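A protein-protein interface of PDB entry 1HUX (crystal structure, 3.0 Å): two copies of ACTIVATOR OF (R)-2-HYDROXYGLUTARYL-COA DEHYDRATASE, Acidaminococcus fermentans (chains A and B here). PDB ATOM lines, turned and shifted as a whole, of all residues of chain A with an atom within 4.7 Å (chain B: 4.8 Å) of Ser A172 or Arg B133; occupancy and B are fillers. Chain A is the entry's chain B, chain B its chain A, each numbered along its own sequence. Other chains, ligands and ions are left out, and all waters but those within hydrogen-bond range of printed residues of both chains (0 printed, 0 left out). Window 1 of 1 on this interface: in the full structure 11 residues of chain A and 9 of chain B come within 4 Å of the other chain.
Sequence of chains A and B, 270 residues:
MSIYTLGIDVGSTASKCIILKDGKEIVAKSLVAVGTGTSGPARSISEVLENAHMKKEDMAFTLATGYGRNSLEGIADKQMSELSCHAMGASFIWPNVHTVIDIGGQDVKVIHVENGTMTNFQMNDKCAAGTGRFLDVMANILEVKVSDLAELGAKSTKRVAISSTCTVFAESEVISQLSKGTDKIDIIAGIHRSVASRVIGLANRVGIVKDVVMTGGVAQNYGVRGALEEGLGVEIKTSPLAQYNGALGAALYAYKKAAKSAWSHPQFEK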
ATOM      1  N   VAL A 168       5.089  10.187  -9.935  1.00  0.00           N
ATOM      2  CA  VAL A 168       3.678   9.937  -9.597  1.00  0.00           C
ATOM      3  C   VAL A 168       3.306   8.466  -9.693  1.00  0.00           C
ATOM      4  O   VAL A 168       2.725   7.891  -8.770  1.00  0.00           O
ATOM      5  CB  VAL A 168       2.715  10.719 -10.493  1.00  0.00           C
ATOM      6  CG1 VAL A 168       1.279  10.438 -10.077  1.00  0.00           C
ATOM      7  CG2 VAL A 168       3.024  12.215 -10.407  1.00  0.00           C
ATOM      8  N   PHE A 169       3.646   7.844 -10.808  1.00  0.00           N
ATOM      9  CA  PHE A 169       3.350   6.433 -10.957  1.00  0.00           C
ATOM     10  C   PHE A 169       4.201   5.624  -9.981  1.00  0.00           C
ATOM     11  O   PHE A 169       3.690   4.720  -9.321  1.00  0.00           O
ATOM     12  CB  PHE A 169       3.582   6.008 -12.412  1.00  0.00           C
ATOM     13  CG  PHE A 169       2.578   6.613 -13.379  1.00  0.00           C
ATOM     14  CD1 PHE A 169       2.916   6.854 -14.715  1.00  0.00           C
ATOM     15  CD2 PHE A 169       1.305   6.982 -12.943  1.00  0.00           C
ATOM     16  CE1 PHE A 169       1.997   7.464 -15.600  1.00  0.00           C
ATOM     17  CE2 PHE A 169       0.382   7.589 -13.822  1.00  0.00           C
ATOM     18  CZ  PHE A 169       0.733   7.829 -15.149  1.00  0.00           C
ATOM     19  N   ALA A 170       5.483   5.963  -9.862  1.00  0.00           N
ATOM     20  CA  ALA A 170       6.368   5.240  -8.940  1.00  0.00           C
ATOM     21  C   ALA A 170       5.862   5.373  -7.502  1.00  0.00           C
ATOM     22  O   ALA A 170       6.104   4.501  -6.670  1.00  0.00           O
ATOM     23  CB  ALA A 170       7.813   5.763  -9.049  1.00  0.00           C
ATOM     24  N   GLU A 171       5.161   6.464  -7.213  1.00  0.00           N
ATOM     25  CA  GLU A 171       4.626   6.658  -5.880  1.00  0.00           C
ATOM     26  C   GLU A 171       3.641   5.517  -5.593  1.00  0.00           C
ATOM     27  O   GLU A 171       3.725   4.848  -4.555  1.00  0.00           O
ATOM     28  CB  GLU A 171       3.939   8.019  -5.783  1.00  0.00           C
ATOM     29  CG  GLU A 171       3.198   8.241  -4.483  1.00  0.00           C
ATOM     30  CD  GLU A 171       2.816   9.693  -4.268  1.00  0.00           C
ATOM     31  OE1 GLU A 171       2.403  10.357  -5.244  1.00  0.00           O
ATOM     32  OE2 GLU A 171       2.920  10.169  -3.117  1.00  0.00           O
ATOM     33  N   SER A 172       2.724   5.280  -6.528  1.00  0.00           N
ATOM     34  CA  SER A 172       1.753   4.204  -6.378  1.00  0.00           C
ATOM     35  C   SER A 172       2.463   2.871  -6.258  1.00  0.00           C
ATOM     36  O   SER A 172       2.077   2.030  -5.453  1.00  0.00           O
ATOM     37  CB  SER A 172       0.830   4.153  -7.581  1.00  0.00           C
ATOM     38  OG  SER A 172       0.133   5.371  -7.710  1.00  0.00           O
ATOM     39  N   GLU A 173       3.495   2.670  -7.070  1.00  0.00           N
ATOM     40  CA  GLU A 173       4.239   1.424  -7.011  1.00  0.00           C
ATOM     41  C   GLU A 173       4.696   1.209  -5.578  1.00  0.00           C
ATOM     42  O   GLU A 173       4.436   0.162  -4.982  1.00  0.00           O
ATOM     43  CB  GLU A 173       5.473   1.462  -7.921  1.00  0.00           C
ATOM     44  CG  GLU A 173       5.251   0.985  -9.351  1.00  0.00           C
ATOM     45  CD  GLU A 173       6.540   0.506 -10.010  1.00  0.00           C
ATOM     46  OE1 GLU A 173       7.139  -0.477  -9.518  1.00  0.00           O
ATOM     47  OE2 GLU A 173       6.955   1.110 -11.018  1.00  0.00           O
ATOM     48  N   VAL A 174       5.377   2.207  -5.023  1.00  0.00           N
ATOM     49  CA  VAL A 174       5.878   2.098  -3.666  1.00  0.00           C
ATOM     50  C   VAL A 174       4.755   1.738  -2.701  1.00  0.00           C
ATOM     51  O   VAL A 174       4.928   0.902  -1.811  1.00  0.00           O
ATOM     52  CB  VAL A 174       6.561   3.404  -3.238  1.00  0.00           C
ATOM     53  CG1 VAL A 174       6.948   3.340  -1.762  1.00  0.00           C
ATOM     54  CG2 VAL A 174       7.796   3.615  -4.088  1.00  0.00           C
ATOM     55  N   ILE A 175       3.599   2.360  -2.892  1.00  0.00           N
ATOM     56  CA  ILE A 175       2.436   2.090  -2.054  1.00  0.00           C
ATOM     57  C   ILE A 175       2.040   0.618  -2.206  1.00  0.00           C
ATOM     58  O   ILE A 175       1.815  -0.091  -1.221  1.00  0.00           O
ATOM     59  CB  ILE A 175       1.234   2.970  -2.482  1.00  0.00           C
ATOM     60  CG1 ILE A 175       1.556   4.445  -2.237  1.00  0.00           C
ATOM     61  CG2 ILE A 175      -0.028   2.542  -1.739  1.00  0.00           C
ATOM     62  CD1 ILE A 175       0.492   5.389  -2.759  1.00  0.00           C
ATOM     63  N   SER A 176       1.963   0.180  -3.460  1.00  0.00           N
ATOM     64  CA  SER A 176       1.593  -1.186  -3.795  1.00  0.00           C
ATOM     65  C   SER A 176       2.616  -2.210  -3.316  1.00  0.00           C
ATOM     66  O   SER A 176       2.252  -3.331  -2.983  1.00  0.00           O
ATOM     67  CB  SER A 176       1.399  -1.322  -5.308  1.00  0.00           C
ATOM     68  OG  SER A 176       1.046  -2.651  -5.657  1.00  0.00           O
ATOM     69  N   GLY B 105      -7.380   7.851 -17.429  1.00  0.00           N
ATOM     70  CA  GLY B 105      -6.460   7.932 -16.312  1.00  0.00           C
ATOM     71  C   GLY B 105      -5.192   7.246 -16.776  1.00  0.00           C
ATOM     72  O   GLY B 105      -5.244   6.349 -17.626  1.00  0.00           O
ATOM     73  N   GLN B 106      -4.052   7.679 -16.259  1.00  0.00           N
ATOM     74  CA  GLN B 106      -2.763   7.077 -16.620  1.00  0.00           C
ATOM     75  C   GLN B 106      -2.250   7.077 -18.075  1.00  0.00           C
ATOM     76  O   GLN B 106      -1.215   6.451 -18.361  1.00  0.00           O
ATOM     77  CB  GLN B 106      -2.722   5.655 -16.083  1.00  0.00           C
ATOM     78  CG  GLN B 106      -2.599   5.623 -14.586  1.00  0.00           C
ATOM     79  CD  GLN B 106      -3.020   4.303 -13.998  1.00  0.00           C
ATOM     80  OE1 GLN B 106      -2.538   3.245 -14.418  1.00  0.00           O
ATOM     81  NE2 GLN B 106      -3.922   4.350 -13.010  1.00  0.00           N
ATOM     82  N   ALA B 128       2.694  11.231 -16.273  1.00  0.00           N
ATOM     83  CA  ALA B 128       1.380  11.426 -15.669  1.00  0.00           C
ATOM     84  C   ALA B 128       0.768  12.747 -16.121  1.00  0.00           C
ATOM     85  O   ALA B 128      -0.415  12.988 -15.908  1.00  0.00           O
ATOM     86  CB  ALA B 128       1.504  11.412 -14.153  1.00  0.00           C
ATOM     87  N   THR B 131      -2.744  13.455 -18.223  1.00  0.00           N
ATOM     88  CA  THR B 131      -3.659  12.342 -17.983  1.00  0.00           C
ATOM     89  C   THR B 131      -4.686  12.731 -16.918  1.00  0.00           C
ATOM     90  O   THR B 131      -4.581  13.781 -16.293  1.00  0.00           O
ATOM     91  CB  THR B 131      -2.936  11.125 -17.448  1.00  0.00           C
ATOM     92  OG1 THR B 131      -2.671  11.340 -16.056  1.00  0.00           O
ATOM     93  CG2 THR B 131      -1.630  10.890 -18.203  1.00  0.00           C
ATOM     94  N   GLY B 132      -5.676  11.876 -16.713  1.00  0.00           N
ATOM     95  CA  GLY B 132      -6.694  12.182 -15.727  1.00  0.00           C
ATOM     96  C   GLY B 132      -6.081  12.112 -14.343  1.00  0.00           C
ATOM     97  O   GLY B 132      -6.655  12.598 -13.358  1.00  0.00           O
ATOM     98  N   ARG B 133      -4.902  11.498 -14.278  1.00  0.00           N
ATOM     99  CA  ARG B 133      -4.183  11.346 -13.027  1.00  0.00           C
ATOM    100  C   ARG B 133      -3.621  12.710 -12.615  1.00  0.00           C
ATOM    101  O   ARG B 133      -3.461  13.021 -11.432  1.00  0.00           O
ATOM    102  CB  ARG B 133      -3.062  10.334 -13.216  1.00  0.00           C
ATOM    103  CG  ARG B 133      -2.246  10.098 -11.977  1.00  0.00           C
ATOM    104  CD  ARG B 133      -3.128   9.719 -10.796  1.00  0.00           C
ATOM    105  NE  ARG B 133      -2.303   9.222  -9.710  1.00  0.00           N
ATOM    106  CZ  ARG B 133      -1.585   8.102  -9.787  1.00  0.00           C
ATOM    107  NH1 ARG B 133      -1.604   7.360 -10.896  1.00  0.00           N
ATOM    108  NH2 ARG B 133      -0.820   7.737  -8.764  1.00  0.00           N
ATOM    109  N   PHE B 134      -3.315  13.519 -13.622  1.00  0.00           N
ATOM    110  CA  PHE B 134      -2.812  14.867 -13.400  1.00  0.00           C
ATOM    111  C   PHE B 134      -3.936  15.596 -12.663  1.00  0.00           C
ATOM    112  O   PHE B 134      -3.726  16.166 -11.595  1.00  0.00           O
ATOM    113  CB  PHE B 134      -2.523  15.545 -14.756  1.00  0.00           C
ATOM    114  CG  PHE B 134      -2.088  16.977 -14.645  1.00  0.00           C
ATOM    115  CD1 PHE B 134      -0.810  17.300 -14.211  1.00  0.00           C
ATOM    116  CD2 PHE B 134      -2.973  18.002 -14.933  1.00  0.00           C
ATOM    117  CE1 PHE B 134      -0.402  18.620 -14.050  1.00  0.00           C
ATOM    118  CE2 PHE B 134      -2.591  19.341 -14.783  1.00  0.00           C
ATOM    119  CZ  PHE B 134      -1.295  19.651 -14.337  1.00  0.00           C
ATOM    120  N   LEU B 135      -5.135  15.530 -13.242  1.00  0.00           N
ATOM    121  CA  LEU B 135      -6.328  16.170 -12.689  1.00  0.00           C
ATOM    122  C   LEU B 135      -6.681  15.680 -11.293  1.00  0.00           C
ATOM    123  O   LEU B 135      -7.246  16.423 -10.499  1.00  0.00           O
ATOM    124  CB  LEU B 135      -7.531  15.955 -13.619  1.00  0.00           C
ATOM    125  CG  LEU B 135      -7.452  16.619 -14.992  1.00  0.00           C
ATOM    126  CD1 LEU B 135      -8.612  16.187 -15.871  1.00  0.00           C
ATOM    127  CD2 LEU B 135      -7.442  18.136 -14.807  1.00  0.00           C
ATOM    128  N   ASP B 136      -6.357  14.429 -10.992  1.00  0.00           N
ATOM    129  CA  ASP B 136      -6.657  13.894  -9.667  1.00  0.00           C
ATOM    130  C   ASP B 136      -5.774  14.576  -8.653  1.00  0.00           C
ATOM    131  O   ASP B 136      -6.256  15.212  -7.712  1.00  0.00           O
ATOM    132  CB  ASP B 136      -6.422  12.383  -9.615  1.00  0.00           C
ATOM    133  CG  ASP B 136      -7.571  11.598 -10.203  1.00  0.00           C
ATOM    134  OD1 ASP B 136      -8.722  11.786  -9.741  1.00  0.00           O
ATOM    135  OD2 ASP B 136      -7.318  10.797 -11.126  1.00  0.00           O
ATOM    136  N   VAL B 137      -4.470  14.446  -8.859  1.00  0.00           N
ATOM    137  CA  VAL B 137      -3.489  15.059  -7.972  1.00  0.00           C
ATOM    138  C   VAL B 137      -3.771  16.550  -7.730  1.00  0.00           C
ATOM    139  O   VAL B 137      -3.421  17.087  -6.685  1.00  0.00           O
ATOM    140  CB  VAL B 137      -2.064  14.901  -8.543  1.00  0.00           C
ATOM    141  CG1 VAL B 137      -1.073  15.671  -7.680  1.00  0.00           C
ATOM    142  CG2 VAL B 137      -1.686  13.409  -8.621  1.00  0.00           C
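The backbone NH (N) of Arg B133 sits at hydrogen-bond distance from the side-chain hydroxyl (OG1) of Thr B131, 2.9 Å away.
The backbone carbonyl oxygen (O) of Ala B128 sits at hydrogen-bond distance from the side-chain hydroxyl (OG1) of Thr B131.
The side-chain hydroxyl (OG) of Ser A172 is in hydrogen-bond range of the guanidinium group (NH2) of Arg B133, 2.8 Å away.
Of the 10 printed residues of chain B, 3 touch a printed residue of chain A.
Printed residues of chain B that touch a printed residue of chain A: Gln B106, Ala B128 and Arg B133.
Along chain B the printed residues that touch a printed residue of chain A span positions 106 to 133.
Printed residues of chain A that touch a printed residue of chain B: Val A168, Phe A169 and Ser A172.
Hydrophobic or aromatic side chains of chain A within 4 Å of the printed part of chain B: Val A168 and Phe A169.
Among the printed residues, no Asp or Glu carboxylate lies within 4 Å of a Lys or Arg side-chain nitrogen of the other chain.
No position is printed for both chains.
Of the 6 pairs that touch across the chains among the printed residues, none has its exchanged pair printed and touching as well.
Val A168 touches Ala B128.
NH2 of Arg B133 touches O of Val A168, at 3.5 Å.
Phe A169 touches Gln B106.
Phe A169 touches Ala B128.
Phe A169 touches Arg B133.
Ser A172 touches just one residue of chain B: Arg B133 (2.8 Å).
Of chain A, only Val A168, Phe A169 and Ser A172 come within 4 Å of Arg B133.
Of the printed residues of chain B, Phe A169 touches Gln B106 (3.7 Å), Ala B128 (3.7 Å) and Arg B133 (3.5 Å).
Printed residues of chain B within 4 Å of Val A168: Ala B128 and Arg B133.
Asp B136 touches none of the printed residues of chain A.
Ala A170 touches none of the printed residues of chain B.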
